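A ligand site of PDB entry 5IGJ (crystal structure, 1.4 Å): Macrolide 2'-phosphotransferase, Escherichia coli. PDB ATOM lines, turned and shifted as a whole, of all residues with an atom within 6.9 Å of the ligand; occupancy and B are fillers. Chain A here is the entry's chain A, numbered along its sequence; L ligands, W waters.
Water W3 lies within hydrogen-bond range of O4 of the ligand (2.7 Å) and O of Gly 204 (2.7 Å).
Water W1 lies within hydrogen-bond range of NH1 of Arg 52 (2.8 Å), O1 of the ligand (2.8 Å) and OH of Tyr 94 (2.9 Å).
Water W2 bridges N4 of the ligand and N of Thr 101.
The backbone NH (N) of Leu 97 sits at hydrogen-bond distance from an oxygen (O5) of the ligand (3.0 Å).
O1 of the ligand sits at hydrogen-bond distance from OD1 of Asp 219, 2.7 Å away.
A nitrogen (N3) of the ligand is in hydrogen-bond range of the backbone carbonyl oxygen of Leu 97, at 2.7 Å.
OH of Tyr 94 sits at hydrogen-bond distance from N2 of the ligand, at 2.6 Å.
O of Asp 99 is in hydrogen-bond range of N4 of the ligand (2.8 Å).
Merely in contact with the ligand: Val 50 (3.6 Å), Arg 52 (3.7 Å), Met 96 (3.7 Å), His 205 (3.6 Å), Leu 207 (3.8 Å) and Ile 218 (3.5 Å).
Hydrophobic or aromatic side chains within 4 Å of the ligand: Val 50, Tyr 94, Met 96, Leu 97, His 205, Leu 207 and Ile 218.
Ten residues have an atom within 4 Å of the ligand: Val 50, Arg 52, Tyr 94, Met 96, Leu 97, Asp 99, His 205, Leu 207, Ile 218 and Asp 219.
The nearest printed residue that does not touch the ligand is Ile 38 (4.001 Å).
NH1 of Arg 52 lies within salt-bridge range of OD1 of Asp 219 (3.9 Å).
The backbone NH of Met 96 lies within hydrogen-bond range of the backbone carbonyl oxygen of Arg 48 (2.8 Å).
OD2 of Asp 219 lies within hydrogen-bond range of NE2 of His 205, 2.9 Å away.
O of His 205 lies within hydrogen-bond range of N of Ile 218, 2.9 Å away.
The backbone carbonyl oxygen (O) of Tyr 94 is in hydrogen-bond range of the backbone NH (N) of Val 50, 2.8 Å away.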
ATOM      1  N   ASN A  30      -8.230 -33.106  -6.393  1.00  0.00           N
ATOM      2  CA  ASN A  30      -8.038 -34.389  -5.730  1.00  0.00           C
ATOM      3  C   ASN A  30      -9.270 -35.246  -5.966  1.00  0.00           C
ATOM      4  O   ASN A  30     -10.376 -34.922  -5.514  1.00  0.00           O
ATOM      5  CB  ASN A  30      -7.790 -34.186  -4.239  1.00  0.00           C
ATOM      6  CG  ASN A  30      -7.416 -35.466  -3.538  1.00  0.00           C
ATOM      7  OD1 ASN A  30      -7.897 -36.544  -3.880  1.00  0.00           O
ATOM      8  ND2 ASN A  30      -6.556 -35.361  -2.536  1.00  0.00           N
ATOM      9  N   ILE A  38     -12.423 -32.875  -4.632  1.00  0.00           N
ATOM     10  CA  ILE A  38     -11.987 -31.667  -3.922  1.00  0.00           C
ATOM     11  C   ILE A  38     -11.096 -30.899  -4.839  1.00  0.00           C
ATOM     12  O   ILE A  38     -10.088 -31.410  -5.356  1.00  0.00           O
ATOM     13  CB  ILE A  38     -11.226 -31.991  -2.625  1.00  0.00           C
ATOM     14  CG1 ILE A  38     -12.051 -32.920  -1.713  1.00  0.00           C
ATOM     15  CG2 ILE A  38     -10.831 -30.716  -1.903  1.00  0.00           C
ATOM     16  CD1 ILE A  38     -13.314 -32.318  -1.185  1.00  0.00           C
ATOM     17  N   ILE A  40      -9.060 -27.170  -5.241  1.00  0.00           N
ATOM     18  CA  ILE A  40      -8.674 -25.848  -4.765  1.00  0.00           C
ATOM     19  C   ILE A  40      -8.478 -24.984  -5.993  1.00  0.00           C
ATOM     20  O   ILE A  40      -7.618 -25.282  -6.849  1.00  0.00           O
ATOM     21  CB  ILE A  40      -7.428 -25.894  -3.884  1.00  0.00           C
ATOM     22  CG1 ILE A  40      -7.708 -26.763  -2.661  1.00  0.00           C
ATOM     23  CG2 ILE A  40      -7.021 -24.472  -3.486  1.00  0.00           C
ATOM     24  CD1 ILE A  40      -6.558 -26.847  -1.686  1.00  0.00           C
ATOM     25  N   ARG A  48      -8.059 -18.060  -3.208  1.00  0.00           N
ATOM     26  CA  ARG A  48      -8.314 -19.475  -3.427  1.00  0.00           C
ATOM     27  C   ARG A  48      -9.551 -19.910  -2.647  1.00  0.00           C
ATOM     28  O   ARG A  48      -9.791 -19.458  -1.528  1.00  0.00           O
ATOM     29  CB  ARG A  48      -7.135 -20.288  -2.993  1.00  0.00           C
ATOM     30  CG  ARG A  48      -5.936 -19.978  -3.852  1.00  0.00           C
ATOM     31  CD  ARG A  48      -5.038 -21.150  -3.911  1.00  0.00           C
ATOM     32  NE  ARG A  48      -4.422 -21.408  -2.629  1.00  0.00           N
ATOM     33  CZ  ARG A  48      -3.609 -22.435  -2.376  1.00  0.00           C
ATOM     34  NH1 ARG A  48      -3.317 -23.312  -3.341  1.00  0.00           N
ATOM     35  NH2 ARG A  48      -3.086 -22.589  -1.176  1.00  0.00           N
ATOM     36  N   VAL A  50     -11.993 -23.560  -1.843  1.00  0.00           N
ATOM     37  CA  VAL A  50     -12.137 -25.003  -1.879  1.00  0.00           C
ATOM     38  C   VAL A  50     -13.511 -25.319  -2.422  1.00  0.00           C
ATOM     39  O   VAL A  50     -14.525 -24.779  -1.933  1.00  0.00           O
ATOM     40  CB  VAL A  50     -11.977 -25.614  -0.464  1.00  0.00           C
ATOM     41  CG1 VAL A  50     -12.123 -27.136  -0.519  1.00  0.00           C
ATOM     42  CG2 VAL A  50     -10.639 -25.228   0.115  1.00  0.00           C
ATOM     43  N   ARG A  52     -15.916 -28.427  -2.831  1.00  0.00           N
ATOM     44  CA  ARG A  52     -16.160 -29.746  -2.296  1.00  0.00           C
ATOM     45  C   ARG A  52     -17.388 -30.256  -3.051  1.00  0.00           C
ATOM     46  O   ARG A  52     -18.494 -29.795  -2.830  1.00  0.00           O
ATOM     47  CB  ARG A  52     -16.364 -29.592  -0.796  1.00  0.00           C
ATOM     48  CG  ARG A  52     -16.797 -30.767  -0.006  1.00  0.00           C
ATOM     49  CD  ARG A  52     -16.819 -30.319   1.478  1.00  0.00           C
ATOM     50  NE  ARG A  52     -17.092 -31.429   2.370  1.00  0.00           N
ATOM     51  CZ  ARG A  52     -16.188 -32.317   2.738  1.00  0.00           C
ATOM     52  NH1 ARG A  52     -14.934 -32.208   2.323  1.00  0.00           N
ATOM     53  NH2 ARG A  52     -16.533 -33.321   3.543  1.00  0.00           N
ATOM     54  N   PRO A  82     -14.361 -23.900   8.080  1.00  0.00           N
ATOM     55  CA  PRO A  82     -14.789 -23.513   6.736  1.00  0.00           C
ATOM     56  C   PRO A  82     -16.069 -22.678   6.766  1.00  0.00           C
ATOM     57  O   PRO A  82     -17.039 -23.009   7.487  1.00  0.00           O
ATOM     58  CB  PRO A  82     -15.011 -24.866   6.040  1.00  0.00           C
ATOM     59  CG  PRO A  82     -14.025 -25.783   6.715  1.00  0.00           C
ATOM     60  CD  PRO A  82     -14.130 -25.346   8.178  1.00  0.00           C
ATOM     61  N   TYR A  94     -16.052 -22.827  -0.099  1.00  0.00           N
ATOM     62  CA  TYR A  94     -15.627 -21.910   0.955  1.00  0.00           C
ATOM     63  C   TYR A  94     -14.293 -21.312   0.612  1.00  0.00           C
ATOM     64  O   TYR A  94     -13.454 -21.950  -0.043  1.00  0.00           O
ATOM     65  CB  TYR A  94     -15.572 -22.595   2.312  1.00  0.00           C
ATOM     66  CG  TYR A  94     -14.752 -23.860   2.457  1.00  0.00           C
ATOM     67  CD1 TYR A  94     -15.311 -25.102   2.148  1.00  0.00           C
ATOM     68  CD2 TYR A  94     -13.449 -23.827   2.911  1.00  0.00           C
ATOM     69  CE1 TYR A  94     -14.600 -26.269   2.350  1.00  0.00           C
ATOM     70  CE2 TYR A  94     -12.707 -25.016   3.093  1.00  0.00           C
ATOM     71  CZ  TYR A  94     -13.311 -26.227   2.806  1.00  0.00           C
ATOM     72  OH  TYR A  94     -12.613 -27.404   3.005  1.00  0.00           O
ATOM     73  N   PRO A  95     -14.028 -20.083   1.083  1.00  0.00           N
ATOM     74  CA  PRO A  95     -12.687 -19.532   0.889  1.00  0.00           C
ATOM     75  C   PRO A  95     -11.669 -20.421   1.582  1.00  0.00           C
ATOM     76  O   PRO A  95     -11.897 -20.875   2.704  1.00  0.00           O
ATOM     77  CB  PRO A  95     -12.750 -18.158   1.579  1.00  0.00           C
ATOM     78  CG  PRO A  95     -14.177 -17.884   1.777  1.00  0.00           C
ATOM     79  CD  PRO A  95     -14.944 -19.169   1.779  1.00  0.00           C
ATOM     80  N   MET A  96     -10.559 -20.706   0.912  1.00  0.00           N
ATOM     81  CA  MET A  96      -9.579 -21.580   1.519  1.00  0.00           C
ATOM     82  C   MET A  96      -9.051 -20.930   2.773  1.00  0.00           C
ATOM     83  O   MET A  96      -8.778 -19.739   2.808  1.00  0.00           O
ATOM     84  CB  MET A  96      -8.415 -21.877   0.573  1.00  0.00           C
ATOM     85  CG  MET A  96      -7.488 -22.964   1.108  1.00  0.00           C
ATOM     86  SD  MET A  96      -6.054 -23.163   0.056  1.00  0.00           S
ATOM     87  CE  MET A  96      -5.104 -24.356   0.989  1.00  0.00           C
ATOM     88  N   LEU A  97      -8.890 -21.743   3.803  1.00  0.00           N
ATOM     89  CA  LEU A  97      -8.173 -21.357   5.009  1.00  0.00           C
ATOM     90  C   LEU A  97      -6.724 -21.647   4.703  1.00  0.00           C
ATOM     91  O   LEU A  97      -6.320 -22.812   4.594  1.00  0.00           O
ATOM     92  CB  LEU A  97      -8.706 -22.136   6.214  1.00  0.00           C
ATOM     93  CG  LEU A  97     -10.193 -21.989   6.465  1.00  0.00           C
ATOM     94  CD1 LEU A  97     -10.709 -22.944   7.568  1.00  0.00           C
ATOM     95  CD2 LEU A  97     -10.551 -20.561   6.817  1.00  0.00           C
ATOM     96  N   GLU A  98      -5.948 -20.607   4.450  1.00  0.00           N
ATOM     97  CA  GLU A  98      -4.647 -20.794   3.820  1.00  0.00           C
ATOM     98  C   GLU A  98      -3.581 -21.398   4.720  1.00  0.00           C
ATOM     99  O   GLU A  98      -2.587 -21.937   4.223  1.00  0.00           O
ATOM    100  CB  GLU A  98      -4.169 -19.478   3.190  1.00  0.00           C
ATOM    101  CG  GLU A  98      -4.979 -19.089   1.942  1.00  0.00           C
ATOM    102  CD  GLU A  98      -4.604 -19.894   0.707  1.00  0.00           C
ATOM    103  OE1 GLU A  98      -3.821 -20.872   0.832  1.00  0.00           O
ATOM    104  OE2 GLU A  98      -5.101 -19.570  -0.393  1.00  0.00           O
ATOM    105  N   ASP A  99      -3.813 -21.395   6.028  1.00  0.00           N
ATOM    106  CA  ASP A  99      -2.867 -22.031   6.934  1.00  0.00           C
ATOM    107  C   ASP A  99      -2.707 -23.517   6.614  1.00  0.00           C
ATOM    108  O   ASP A  99      -3.657 -24.200   6.238  1.00  0.00           O
ATOM    109  CB  ASP A  99      -3.323 -21.884   8.391  1.00  0.00           C
ATOM    110  CG  ASP A  99      -3.010 -20.523   8.989  1.00  0.00           C
ATOM    111  OD1 ASP A  99      -2.416 -19.665   8.304  1.00  0.00           O
ATOM    112  OD2 ASP A  99      -3.388 -20.307  10.152  1.00  0.00           O
ATOM    113  N   SER A 100      -1.504 -24.038   6.832  1.00  0.00           N
ATOM    114  CA  SER A 100      -1.224 -25.430   6.547  1.00  0.00           C
ATOM    115  C   SER A 100      -1.972 -26.361   7.484  1.00  0.00           C
ATOM    116  O   SER A 100      -2.193 -26.024   8.641  1.00  0.00           O
ATOM    117  CB  SER A 100       0.270 -25.705   6.761  1.00  0.00           C
ATOM    118  OG  SER A 100       0.603 -27.020   6.347  1.00  0.00           O
ATOM    119  N   THR A 101      -2.309 -27.548   6.994  1.00  0.00           N
ATOM    120  CA  THR A 101      -2.618 -28.653   7.894  1.00  0.00           C
ATOM    121  C   THR A 101      -1.393 -29.026   8.741  1.00  0.00           C
ATOM    122  O   THR A 101      -0.247 -28.698   8.369  1.00  0.00           O
ATOM    123  CB  THR A 101      -3.155 -29.876   7.107  1.00  0.00           C
ATOM    124  OG1 THR A 101      -2.266 -30.169   6.016  1.00  0.00           O
ATOM    125  CG2 THR A 101      -4.535 -29.598   6.550  1.00  0.00           C
ATOM    126  N   ILE A 105       0.871 -34.344   3.179  1.00  0.00           N
ATOM    127  CA  ILE A 105       0.973 -35.636   2.473  1.00  0.00           C
ATOM    128  C   ILE A 105       0.584 -35.432   1.019  1.00  0.00           C
ATOM    129  O   ILE A 105      -0.331 -34.660   0.717  1.00  0.00           O
ATOM    130  CB  ILE A 105       0.116 -36.735   3.150  1.00  0.00           C
ATOM    131  CG1 ILE A 105       0.333 -38.113   2.510  1.00  0.00           C
ATOM    132  CG2 ILE A 105      -1.392 -36.372   3.083  1.00  0.00           C
ATOM    133  CD1 ILE A 105      -0.178 -39.252   3.368  1.00  0.00           C
ATOM    134  N   TYR A 202      -7.697 -35.452  13.565  1.00  0.00           N
ATOM    135  CA  TYR A 202      -6.293 -35.852  13.622  1.00  0.00           C
ATOM    136  C   TYR A 202      -5.504 -34.730  12.987  1.00  0.00           C
ATOM    137  O   TYR A 202      -6.093 -33.760  12.510  1.00  0.00           O
ATOM    138  CB  TYR A 202      -6.045 -37.202  12.903  1.00  0.00           C
ATOM    139  CG  TYR A 202      -5.944 -37.143  11.372  1.00  0.00           C
ATOM    140  CD1 TYR A 202      -7.020 -36.721  10.576  1.00  0.00           C
ATOM    141  CD2 TYR A 202      -4.782 -37.483  10.724  1.00  0.00           C
ATOM    142  CE1 TYR A 202      -6.913 -36.672   9.175  1.00  0.00           C
ATOM    143  CE2 TYR A 202      -4.663 -37.433   9.353  1.00  0.00           C
ATOM    144  CZ  TYR A 202      -5.733 -37.021   8.592  1.00  0.00           C
ATOM    145  OH  TYR A 202      -5.560 -37.013   7.203  1.00  0.00           O
ATOM    146  N   GLY A 204      -4.153 -34.197  10.198  1.00  0.00           N
ATOM    147  CA  GLY A 204      -4.533 -33.795   8.853  1.00  0.00           C
ATOM    148  C   GLY A 204      -5.768 -32.931   8.708  1.00  0.00           C
ATOM    149  O   GLY A 204      -6.039 -32.376   7.634  1.00  0.00           O
ATOM    150  N   HIS A 205      -6.541 -32.785   9.794  1.00  0.00           N
ATOM    151  CA  HIS A 205      -7.735 -31.941   9.786  1.00  0.00           C
ATOM    152  C   HIS A 205      -7.603 -30.770  10.731  1.00  0.00           C
ATOM    153  O   HIS A 205      -8.590 -30.091  10.991  1.00  0.00           O
ATOM    154  CB  HIS A 205      -8.957 -32.782  10.159  1.00  0.00           C
ATOM    155  CG  HIS A 205      -9.333 -33.777   9.097  1.00  0.00           C
ATOM    156  ND1 HIS A 205     -10.150 -34.852   9.351  1.00  0.00           N
ATOM    157  CD2 HIS A 205      -9.006 -33.838   7.796  1.00  0.00           C
ATOM    158  CE1 HIS A 205     -10.314 -35.548   8.232  1.00  0.00           C
ATOM    159  NE2 HIS A 205      -9.622 -34.954   7.279  1.00  0.00           N
ATOM    160  N   LEU A 207      -5.557 -27.143  11.271  1.00  0.00           N
ATOM    161  CA  LEU A 207      -4.735 -26.118  10.650  1.00  0.00           C
ATOM    162  C   LEU A 207      -3.887 -25.394  11.690  1.00  0.00           C
ATOM    163  O   LEU A 207      -4.297 -25.219  12.845  1.00  0.00           O
ATOM    164  CB  LEU A 207      -5.598 -25.073   9.933  1.00  0.00           C
ATOM    165  CG  LEU A 207      -6.601 -25.621   8.930  1.00  0.00           C
ATOM    166  CD1 LEU A 207      -7.303 -24.498   8.178  1.00  0.00           C
ATOM    167  CD2 LEU A 207      -5.962 -26.606   7.960  1.00  0.00           C
ATOM    168  N   ILE A 218     -10.786 -28.490   9.950  1.00  0.00           N
ATOM    169  CA  ILE A 218     -11.541 -28.705   8.723  1.00  0.00           C
ATOM    170  C   ILE A 218     -12.166 -30.092   8.721  1.00  0.00           C
ATOM    171  O   ILE A 218     -11.912 -30.900   9.623  1.00  0.00           O
ATOM    172  CB  ILE A 218     -10.648 -28.537   7.477  1.00  0.00           C
ATOM    173  CG1 ILE A 218      -9.517 -29.553   7.516  1.00  0.00           C
ATOM    174  CG2 ILE A 218     -10.116 -27.087   7.429  1.00  0.00           C
ATOM    175  CD1 ILE A 218      -8.618 -29.531   6.297  1.00  0.00           C
ATOM    176  N   ASP A 219     -12.987 -30.361   7.712  1.00  0.00           N
ATOM    177  CA  ASP A 219     -13.557 -31.692   7.448  1.00  0.00           C
ATOM    178  C   ASP A 219     -14.432 -32.180   8.613  1.00  0.00           C
ATOM    179  O   ASP A 219     -14.132 -33.140   9.281  1.00  0.00           O
ATOM    180  CB  ASP A 219     -12.444 -32.707   7.084  1.00  0.00           C
ATOM    181  CG  ASP A 219     -11.831 -32.465   5.701  1.00  0.00           C
ATOM    182  OD1 ASP A 219     -12.171 -31.518   4.997  1.00  0.00           O
ATOM    183  OD2 ASP A 219     -10.976 -33.281   5.309  1.00  0.00           O
HETATM  184  O1  LIG L   1     -11.283 -31.423   2.439  1.00  0.00           O
HETATM  185  C1  LIG L   1     -10.401 -32.410   1.896  1.00  0.00           C
HETATM  186  C2  LIG L   1      -8.936 -32.130   2.148  1.00  0.00           C
HETATM  187  O2  LIG L   1      -8.505 -30.955   1.388  1.00  0.00           O
HETATM  188  C3  LIG L   1      -8.521 -31.823   3.591  1.00  0.00           C
HETATM  189  O3  LIG L   1      -8.382 -32.970   4.407  1.00  0.00           O
HETATM  190  C4  LIG L   1      -7.253 -30.998   3.408  1.00  0.00           C
HETATM  191  O4  LIG L   1      -6.131 -31.770   3.012  1.00  0.00           O
HETATM  192  C5  LIG L   1      -7.698 -30.160   2.232  1.00  0.00           C
HETATM  193  N1  LIG L   1      -8.338 -28.884   2.590  1.00  0.00           N
HETATM  194  C6  LIG L   1      -9.644 -28.719   2.438  1.00  0.00           C
HETATM  195  N2  LIG L   1      -9.973 -27.498   2.881  1.00  0.00           N
HETATM  196  C7  LIG L   1      -8.810 -26.890   3.315  1.00  0.00           C
HETATM  197  C8  LIG L   1      -8.488 -25.616   3.856  1.00  0.00           C
HETATM  198  O5  LIG L   1      -9.423 -24.660   4.022  1.00  0.00           O
HETATM  199  N3  LIG L   1      -7.229 -25.317   4.194  1.00  0.00           N
HETATM  200  C9  LIG L   1      -6.240 -26.223   4.016  1.00  0.00           C
HETATM  201  N4  LIG L   1      -4.937 -25.847   4.389  1.00  0.00           N
HETATM  202  N5  LIG L   1      -6.480 -27.454   3.494  1.00  0.00           N
HETATM  203  C10 LIG L   1      -7.751 -27.768   3.135  1.00  0.00           C
HETATM  204  O   HOH W   1     -13.508 -29.887   1.689  1.00  0.00           O
HETATM  205  O   HOH W   2      -2.553 -27.362   3.836  1.00  0.00           O
HETATM  206  O   HOH W   3      -5.093 -33.116   5.165  1.00  0.00           O
HETATM  207  O   HOH W   4      -7.391 -35.125   3.362  1.00  0.00           O
HETATM  208  O   HOH W   5      -4.271 -28.885   2.373  1.00  0.00           O
HETATM  209  O   HOH W   6      -7.316 -31.748  -1.282  1.00  0.00           O
